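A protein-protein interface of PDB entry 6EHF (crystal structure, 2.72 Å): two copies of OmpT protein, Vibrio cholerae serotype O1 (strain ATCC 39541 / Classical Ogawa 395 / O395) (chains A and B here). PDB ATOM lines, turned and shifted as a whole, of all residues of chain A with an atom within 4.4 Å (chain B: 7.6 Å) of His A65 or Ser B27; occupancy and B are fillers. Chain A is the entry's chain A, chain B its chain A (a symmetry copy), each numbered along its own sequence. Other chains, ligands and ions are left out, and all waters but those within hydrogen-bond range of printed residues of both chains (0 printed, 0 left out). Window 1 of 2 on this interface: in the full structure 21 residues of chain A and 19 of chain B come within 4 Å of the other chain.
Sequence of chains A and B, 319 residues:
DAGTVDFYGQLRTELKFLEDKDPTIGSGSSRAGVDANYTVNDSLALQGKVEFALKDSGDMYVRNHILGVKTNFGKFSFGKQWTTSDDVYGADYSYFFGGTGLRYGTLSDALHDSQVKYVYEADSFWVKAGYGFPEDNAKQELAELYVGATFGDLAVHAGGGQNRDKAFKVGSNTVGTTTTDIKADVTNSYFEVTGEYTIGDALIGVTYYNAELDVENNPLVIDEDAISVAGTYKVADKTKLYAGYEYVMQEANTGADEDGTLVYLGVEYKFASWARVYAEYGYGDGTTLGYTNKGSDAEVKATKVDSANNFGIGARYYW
The side-chain amino group of Lys A80 is in hydrogen-bond range of the backbone carbonyl oxygen of Asp B56 (3.0 Å).
NE2 of His A65 lies within hydrogen-bond range of OG of Ser B30 (2.7 Å).
A ring nitrogen (NE2) of His A65 sits close to the backbone carbonyl oxygen of Arg B12.
OG of Ser B30 lies within hydrogen-bond range of N of Arg B12 (3.1 Å).
The backbone NH (N) of Ser B27 lies within hydrogen-bond range of the side-chain carboxylate (OD2) of Asp B56.
OE1 of Gln B10 is in hydrogen-bond range of NH1 of Arg B12.
The backbone NH (N) of Gly B28 sits at hydrogen-bond distance from the backbone carbonyl oxygen (O) of Arg B12 (3.4 Å).
The backbone carbonyl oxygen of Lys A49 sits at hydrogen-bond distance from the backbone NH of Ile A66 (2.8 Å).
The backbone NH of His A65 is in hydrogen-bond range of the backbone carbonyl oxygen of Lys A80, 2.7 Å away.
Among the printed residues, merely in contact across the chains: His A65 with Ser B27, Ile A66 with Leu B11, Val A62 with Lys B55, His A65 with Leu B54, His A65 with Thr B13, Val A62 with Leu B54 and Lys A49 with Leu B11.
Of the printed residues of chain B, His A65 touches Arg B12, Thr B13, Ser B27, Ser B30 and Leu B54.
Of chain A, only His A65 (3.4 Å) comes within 4 Å of Ser B27.
Printed residues of chain A within 4 Å of Asp B56: Lys A80.
Printed residues of chain A within 4 Å of Leu B54: Val A62 (3.9 Å) and His A65 (3.6 Å).
The nearest printed residue of chain A that does not touch Ser B27 is Gly A79 (5.5 Å).
The nearest printed residue of chain A that does not touch Ser B30 is Val A62 (7.3 Å).
Hydrophobic or aromatic side chains of chain A that line the printed part of chain B: Val A62 and His A65.
Hydrophobic or aromatic side chains of chain B within 4 Å of the printed part of chain A: Leu B11.
Among the printed residues, 10 pairs touch across the chains.
Among the printed residues, no Asp or Glu carboxylate lies within 4 Å of a Lys or Arg side-chain nitrogen of the other chain.
No position is printed for both chains.
Of the 10 pairs that touch across the chains among the printed residues, none has its exchanged pair printed and touching as well.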
ATOM      1  N   LYS A  49      25.770 -15.653  -1.231  1.00  0.00           N
ATOM      2  CA  LYS A  49      26.958 -14.850  -1.442  1.00  0.00           C
ATOM      3  C   LYS A  49      27.325 -14.122  -0.200  1.00  0.00           C
ATOM      4  O   LYS A  49      26.442 -13.749   0.570  1.00  0.00           O
ATOM      5  CB  LYS A  49      26.726 -13.887  -2.564  1.00  0.00           C
ATOM      6  CG  LYS A  49      27.987 -13.420  -3.221  1.00  0.00           C
ATOM      7  CD  LYS A  49      27.605 -12.338  -4.210  1.00  0.00           C
ATOM      8  CE  LYS A  49      28.774 -11.901  -5.065  1.00  0.00           C
ATOM      9  NZ  LYS A  49      28.593 -10.481  -5.470  1.00  0.00           N
ATOM     10  N   VAL A  62      31.914  -7.832   7.083  1.00  0.00           N
ATOM     11  CA  VAL A  62      31.172  -8.281   5.900  1.00  0.00           C
ATOM     12  C   VAL A  62      30.603  -7.119   5.104  1.00  0.00           C
ATOM     13  O   VAL A  62      29.954  -6.261   5.672  1.00  0.00           O
ATOM     14  CB  VAL A  62      30.007  -9.208   6.297  1.00  0.00           C
ATOM     15  CG1 VAL A  62      29.115  -9.532   5.098  1.00  0.00           C
ATOM     16  CG2 VAL A  62      30.558 -10.510   6.860  1.00  0.00           C
ATOM     17  N   ASN A  64      28.770  -7.631   1.673  1.00  0.00           N
ATOM     18  CA  ASN A  64      27.503  -8.084   1.059  1.00  0.00           C
ATOM     19  C   ASN A  64      27.214  -9.434   1.732  1.00  0.00           C
ATOM     20  O   ASN A  64      28.147 -10.207   2.053  1.00  0.00           O
ATOM     21  CB  ASN A  64      27.581  -8.257  -0.507  1.00  0.00           C
ATOM     22  CG  ASN A  64      27.403  -6.949  -1.307  1.00  0.00           C
ATOM     23  OD1 ASN A  64      27.955  -5.911  -0.953  1.00  0.00           O
ATOM     24  ND2 ASN A  64      26.641  -7.017  -2.425  1.00  0.00           N
ATOM     25  N   HIS A  65      25.935  -9.710   1.979  1.00  0.00           N
ATOM     26  CA  HIS A  65      25.534 -11.014   2.501  1.00  0.00           C
ATOM     27  C   HIS A  65      24.159 -11.291   1.930  1.00  0.00           C
ATOM     28  O   HIS A  65      23.207 -10.645   2.324  1.00  0.00           O
ATOM     29  CB  HIS A  65      25.621 -11.025   4.007  1.00  0.00           C
ATOM     30  CG  HIS A  65      25.032 -12.227   4.661  1.00  0.00           C
ATOM     31  ND1 HIS A  65      23.717 -12.609   4.468  1.00  0.00           N
ATOM     32  CD2 HIS A  65      25.555 -13.088   5.576  1.00  0.00           C
ATOM     33  CE1 HIS A  65      23.475 -13.680   5.206  1.00  0.00           C
ATOM     34  NE2 HIS A  65      24.561 -13.972   5.908  1.00  0.00           N
ATOM     35  N   ILE A  66      24.107 -12.251   0.982  1.00  0.00           N
ATOM     36  CA  ILE A  66      23.000 -12.406   0.023  1.00  0.00           C
ATOM     37  C   ILE A  66      22.414 -13.826  -0.070  1.00  0.00           C
ATOM     38  O   ILE A  66      23.131 -14.815  -0.044  1.00  0.00           O
ATOM     39  CB  ILE A  66      23.448 -11.964  -1.380  1.00  0.00           C
ATOM     40  CG1 ILE A  66      24.223 -10.640  -1.272  1.00  0.00           C
ATOM     41  CG2 ILE A  66      22.241 -11.822  -2.296  1.00  0.00           C
ATOM     42  CD1 ILE A  66      24.463  -9.907  -2.572  1.00  0.00           C
ATOM     43  N   PHE A  78      18.116 -11.014  -1.278  1.00  0.00           N
ATOM     44  CA  PHE A  78      17.819 -10.584   0.109  1.00  0.00           C
ATOM     45  C   PHE A  78      19.060 -10.341   1.004  1.00  0.00           C
ATOM     46  O   PHE A  78      20.047 -11.095   0.953  1.00  0.00           O
ATOM     47  CB  PHE A  78      17.031 -11.661   0.842  1.00  0.00           C
ATOM     48  CG  PHE A  78      15.714 -12.011   0.229  1.00  0.00           C
ATOM     49  CD1 PHE A  78      15.648 -12.742  -0.944  1.00  0.00           C
ATOM     50  CD2 PHE A  78      14.538 -11.695   0.882  1.00  0.00           C
ATOM     51  CE1 PHE A  78      14.435 -13.106  -1.479  1.00  0.00           C
ATOM     52  CE2 PHE A  78      13.311 -12.064   0.353  1.00  0.00           C
ATOM     53  CZ  PHE A  78      13.261 -12.767  -0.830  1.00  0.00           C
ATOM     54  N   GLY A  79      18.968  -9.326   1.871  1.00  0.00           N
ATOM     55  CA  GLY A  79      20.021  -9.012   2.854  1.00  0.00           C
ATOM     56  C   GLY A  79      20.934  -7.858   2.478  1.00  0.00           C
ATOM     57  O   GLY A  79      20.573  -6.986   1.666  1.00  0.00           O
ATOM     58  N   LYS A  80      22.127  -7.863   3.064  1.00  0.00           N
ATOM     59  CA  LYS A  80      23.064  -6.762   2.905  1.00  0.00           C
ATOM     60  C   LYS A  80      23.660  -6.696   1.524  1.00  0.00           C
ATOM     61  O   LYS A  80      24.502  -7.526   1.186  1.00  0.00           O
ATOM     62  CB  LYS A  80      24.198  -6.895   3.902  1.00  0.00           C
ATOM     63  CG  LYS A  80      25.206  -5.754   3.853  1.00  0.00           C
ATOM     64  CD  LYS A  80      25.988  -5.679   5.149  1.00  0.00           C
ATOM     65  CE  LYS A  80      26.877  -4.450   5.265  1.00  0.00           C
ATOM     66  NZ  LYS A  80      27.505  -4.495   6.621  1.00  0.00           N
ATOM     67  N   GLN B  10      27.625 -21.966   7.830  1.00  0.00           N
ATOM     68  CA  GLN B  10      26.213 -21.658   7.574  1.00  0.00           C
ATOM     69  C   GLN B  10      26.071 -20.256   7.042  1.00  0.00           C
ATOM     70  O   GLN B  10      26.822 -19.378   7.439  1.00  0.00           O
ATOM     71  CB  GLN B  10      25.400 -21.772   8.850  1.00  0.00           C
ATOM     72  CG  GLN B  10      24.850 -23.149   9.062  1.00  0.00           C
ATOM     73  CD  GLN B  10      24.818 -23.541  10.495  1.00  0.00           C
ATOM     74  OE1 GLN B  10      23.771 -23.571  11.113  1.00  0.00           O
ATOM     75  NE2 GLN B  10      25.976 -23.863  11.028  1.00  0.00           N
ATOM     76  N   LEU B  11      25.100 -20.064   6.149  1.00  0.00           N
ATOM     77  CA  LEU B  11      24.736 -18.752   5.647  1.00  0.00           C
ATOM     78  C   LEU B  11      23.282 -18.543   5.998  1.00  0.00           C
ATOM     79  O   LEU B  11      22.405 -18.718   5.172  1.00  0.00           O
ATOM     80  CB  LEU B  11      24.977 -18.647   4.135  1.00  0.00           C
ATOM     81  CG  LEU B  11      24.990 -17.206   3.571  1.00  0.00           C
ATOM     82  CD1 LEU B  11      26.393 -16.616   3.514  1.00  0.00           C
ATOM     83  CD2 LEU B  11      24.389 -17.138   2.178  1.00  0.00           C
ATOM     84  N   ARG B  12      23.033 -18.158   7.240  1.00  0.00           N
ATOM     85  CA  ARG B  12      21.666 -17.855   7.685  1.00  0.00           C
ATOM     86  C   ARG B  12      21.126 -16.550   7.152  1.00  0.00           C
ATOM     87  O   ARG B  12      21.859 -15.570   7.056  1.00  0.00           O
ATOM     88  CB  ARG B  12      21.548 -17.806   9.198  1.00  0.00           C
ATOM     89  CG  ARG B  12      21.437 -19.187   9.792  1.00  0.00           C
ATOM     90  CD  ARG B  12      22.605 -19.485  10.665  1.00  0.00           C
ATOM     91  NE  ARG B  12      22.200 -19.388  12.062  1.00  0.00           N
ATOM     92  CZ  ARG B  12      22.242 -20.380  12.951  1.00  0.00           C
ATOM     93  NH1 ARG B  12      22.689 -21.577  12.600  1.00  0.00           N
ATOM     94  NH2 ARG B  12      21.882 -20.149  14.228  1.00  0.00           N
ATOM     95  N   THR B  13      19.829 -16.574   6.834  1.00  0.00           N
ATOM     96  CA  THR B  13      19.082 -15.446   6.351  1.00  0.00           C
ATOM     97  C   THR B  13      17.671 -15.543   6.925  1.00  0.00           C
ATOM     98  O   THR B  13      16.999 -16.533   6.743  1.00  0.00           O
ATOM     99  CB  THR B  13      19.048 -15.471   4.843  1.00  0.00           C
ATOM    100  OG1 THR B  13      20.389 -15.417   4.345  1.00  0.00           O
ATOM    101  CG2 THR B  13      18.236 -14.315   4.307  1.00  0.00           C
ATOM    102  N   GLU B  14      17.251 -14.513   7.649  1.00  0.00           N
ATOM    103  CA  GLU B  14      16.057 -14.572   8.463  1.00  0.00           C
ATOM    104  C   GLU B  14      15.171 -13.390   8.115  1.00  0.00           C
ATOM    105  O   GLU B  14      15.667 -12.340   7.701  1.00  0.00           O
ATOM    106  CB  GLU B  14      16.435 -14.611   9.959  1.00  0.00           C
ATOM    107  CG  GLU B  14      17.298 -15.846  10.323  1.00  0.00           C
ATOM    108  CD  GLU B  14      17.867 -15.873  11.746  1.00  0.00           C
ATOM    109  OE1 GLU B  14      17.801 -14.843  12.464  1.00  0.00           O
ATOM    110  OE2 GLU B  14      18.411 -16.942  12.130  1.00  0.00           O
ATOM    111  N   LEU B  15      13.861 -13.600   8.220  1.00  0.00           N
ATOM    112  CA  LEU B  15      12.871 -12.545   8.062  1.00  0.00           C
ATOM    113  C   LEU B  15      11.979 -12.621   9.290  1.00  0.00           C
ATOM    114  O   LEU B  15      11.309 -13.644   9.491  1.00  0.00           O
ATOM    115  CB  LEU B  15      12.080 -12.764   6.779  1.00  0.00           C
ATOM    116  CG  LEU B  15      10.731 -12.060   6.563  1.00  0.00           C
ATOM    117  CD1 LEU B  15      10.801 -10.549   6.790  1.00  0.00           C
ATOM    118  CD2 LEU B  15      10.205 -12.377   5.166  1.00  0.00           C
ATOM    119  N   LYS B  16      11.988 -11.567  10.116  1.00  0.00           N
ATOM    120  CA  LYS B  16      11.386 -11.645  11.441  1.00  0.00           C
ATOM    121  C   LYS B  16      10.377 -10.550  11.723  1.00  0.00           C
ATOM    122  O   LYS B  16      10.612  -9.381  11.428  1.00  0.00           O
ATOM    123  CB  LYS B  16      12.474 -11.607  12.519  1.00  0.00           C
ATOM    124  CG  LYS B  16      13.323 -12.869  12.613  1.00  0.00           C
ATOM    125  CD  LYS B  16      14.642 -12.668  13.357  1.00  0.00           C
ATOM    126  CE  LYS B  16      14.479 -12.690  14.858  1.00  0.00           C
ATOM    127  NZ  LYS B  16      15.512 -11.891  15.584  1.00  0.00           N
ATOM    128  N   THR B  24      12.274  -7.133  10.133  1.00  0.00           N
ATOM    129  CA  THR B  24      13.692  -7.113   9.897  1.00  0.00           C
ATOM    130  C   THR B  24      14.005  -8.105   8.793  1.00  0.00           C
ATOM    131  O   THR B  24      13.412  -9.166   8.756  1.00  0.00           O
ATOM    132  CB  THR B  24      14.502  -7.540  11.145  1.00  0.00           C
ATOM    133  OG1 THR B  24      14.401  -8.960  11.322  1.00  0.00           O
ATOM    134  CG2 THR B  24      14.026  -6.849  12.386  1.00  0.00           C
ATOM    135  N   ILE B  25      14.950  -7.758   7.921  1.00  0.00           N
ATOM    136  CA  ILE B  25      15.663  -8.750   7.117  1.00  0.00           C
ATOM    137  C   ILE B  25      17.136  -8.549   7.305  1.00  0.00           C
ATOM    138  O   ILE B  25      17.623  -7.454   7.644  1.00  0.00           O
ATOM    139  CB  ILE B  25      15.443  -8.708   5.580  1.00  0.00           C
ATOM    140  CG1 ILE B  25      14.823  -7.399   5.112  1.00  0.00           C
ATOM    141  CG2 ILE B  25      14.648  -9.908   5.080  1.00  0.00           C
ATOM    142  CD1 ILE B  25      15.257  -7.040   3.706  1.00  0.00           C
ATOM    143  N   GLY B  26      17.831  -9.645   7.047  1.00  0.00           N
ATOM    144  CA  GLY B  26      19.272  -9.713   7.158  1.00  0.00           C
ATOM    145  C   GLY B  26      19.781 -11.089   7.543  1.00  0.00           C
ATOM    146  O   GLY B  26      19.043 -12.073   7.563  1.00  0.00           O
ATOM    147  N   SER B  27      21.062 -11.148   7.862  1.00  0.00           N
ATOM    148  CA  SER B  27      21.661 -12.371   8.303  1.00  0.00           C
ATOM    149  C   SER B  27      21.052 -12.738   9.631  1.00  0.00           C
ATOM    150  O   SER B  27      20.637 -11.875  10.388  1.00  0.00           O
ATOM    151  CB  SER B  27      23.161 -12.173   8.489  1.00  0.00           C
ATOM    152  OG  SER B  27      23.425 -11.317   9.595  1.00  0.00           O
ATOM    153  N   GLY B  28      20.982 -14.026   9.906  1.00  0.00           N
ATOM    154  CA  GLY B  28      21.003 -14.503  11.278  1.00  0.00           C
ATOM    155  C   GLY B  28      22.474 -14.607  11.627  1.00  0.00           C
ATOM    156  O   GLY B  28      23.328 -13.859  11.090  1.00  0.00           O
ATOM    157  N   SER B  29      22.789 -15.576  12.476  1.00  0.00           N
ATOM    158  CA  SER B  29      24.160 -15.768  12.921  1.00  0.00           C
ATOM    159  C   SER B  29      24.978 -16.594  11.940  1.00  0.00           C
ATOM    160  O   SER B  29      25.460 -17.639  12.303  1.00  0.00           O
ATOM    161  CB  SER B  29      24.178 -16.420  14.307  1.00  0.00           C
ATOM    162  OG  SER B  29      25.494 -16.498  14.832  1.00  0.00           O
ATOM    163  N   SER B  30      25.172 -16.136  10.707  1.00  0.00           N
ATOM    164  CA  SER B  30      26.095 -16.842   9.800  1.00  0.00           C
ATOM    165  C   SER B  30      27.494 -16.967  10.440  1.00  0.00           C
ATOM    166  O   SER B  30      27.962 -16.046  11.119  1.00  0.00           O
ATOM    167  CB  SER B  30      26.196 -16.127   8.434  1.00  0.00           C
ATOM    168  OG  SER B  30      24.907 -15.732   7.959  1.00  0.00           O
ATOM    169  N   ARG B  31      28.140 -18.108  10.236  1.00  0.00           N
ATOM    170  CA  ARG B  31      29.541 -18.321  10.649  1.00  0.00           C
ATOM    171  C   ARG B  31      30.239 -19.231   9.607  1.00  0.00           C
ATOM    172  O   ARG B  31      29.604 -19.680   8.632  1.00  0.00           O
ATOM    173  CB  ARG B  31      29.624 -18.960  12.041  1.00  0.00           C
ATOM    174  CG  ARG B  31      29.302 -20.451  12.072  1.00  0.00           C
ATOM    175  CD  ARG B  31      27.810 -20.787  11.871  1.00  0.00           C
ATOM    176  NE  ARG B  31      27.250 -21.102  13.186  1.00  0.00           N
ATOM    177  CZ  ARG B  31      26.141 -20.605  13.727  1.00  0.00           C
ATOM    178  NH1 ARG B  31      25.335 -19.813  13.050  1.00  0.00           N
ATOM    179  NH2 ARG B  31      25.822 -20.944  14.979  1.00  0.00           N
ATOM    180  N   LEU B  54      30.237 -14.434  10.338  1.00  0.00           N
ATOM    181  CA  LEU B  54      29.946 -13.651   9.133  1.00  0.00           C
ATOM    182  C   LEU B  54      28.612 -12.894   9.311  1.00  0.00           C
ATOM    183  O   LEU B  54      27.821 -12.786   8.356  1.00  0.00           O
ATOM    184  CB  LEU B  54      29.823 -14.519   7.864  1.00  0.00           C
ATOM    185  CG  LEU B  54      30.938 -15.231   7.095  1.00  0.00           C
ATOM    186  CD1 LEU B  54      32.300 -14.689   7.459  1.00  0.00           C
ATOM    187  CD2 LEU B  54      30.881 -16.728   7.336  1.00  0.00           C
ATOM    188  N   LYS B  55      28.362 -12.323  10.496  1.00  0.00           N
ATOM    189  CA  LYS B  55      27.091 -11.604  10.725  1.00  0.00           C
ATOM    190  C   LYS B  55      27.112 -10.352   9.808  1.00  0.00           C
ATOM    191  O   LYS B  55      28.176  -9.917   9.369  1.00  0.00           O
ATOM    192  CB  LYS B  55      26.874 -11.303  12.236  1.00  0.00           C
ATOM    193  N   ASP B  56      25.959  -9.819   9.428  1.00  0.00           N
ATOM    194  CA  ASP B  56      25.949  -8.660   8.517  1.00  0.00           C
ATOM    195  C   ASP B  56      26.137  -7.300   9.226  1.00  0.00           C
ATOM    196  O   ASP B  56      26.009  -6.255   8.559  1.00  0.00           O
ATOM    197  CB  ASP B  56      24.650  -8.622   7.728  1.00  0.00           C
ATOM    198  CG  ASP B  56      23.452  -8.207   8.579  1.00  0.00           C
ATOM    199  OD1 ASP B  56      23.646  -7.487   9.594  1.00  0.00           O
ATOM    200  OD2 ASP B  56      22.311  -8.584   8.218  1.00  0.00           O
ATOM    201  N   SER B  57      26.448  -7.321  10.538  1.00  0.00           N
ATOM    202  CA  SER B  57      26.315  -6.166  11.410  1.00  0.00           C
ATOM    203  C   SER B  57      27.612  -5.508  11.814  1.00  0.00           C
ATOM    204  O   SER B  57      27.880  -4.366  11.398  1.00  0.00           O
ATOM    205  CB  SER B  57      25.523  -6.526  12.645  1.00  0.00           C
ATOM    206  OG  SER B  57      24.738  -7.657  12.332  1.00  0.00           O
ATOM    207  N   ALA B 315      16.026 -19.233   6.322  1.00  0.00           N
ATOM    208  CA  ALA B 315      16.571 -19.909   5.145  1.00  0.00           C
ATOM    209  C   ALA B 315      18.099 -19.963   5.236  1.00  0.00           C
ATOM    210  O   ALA B 315      18.783 -18.948   5.123  1.00  0.00           O
ATOM    211  CB  ALA B 315      16.142 -19.216   3.868  1.00  0.00           C
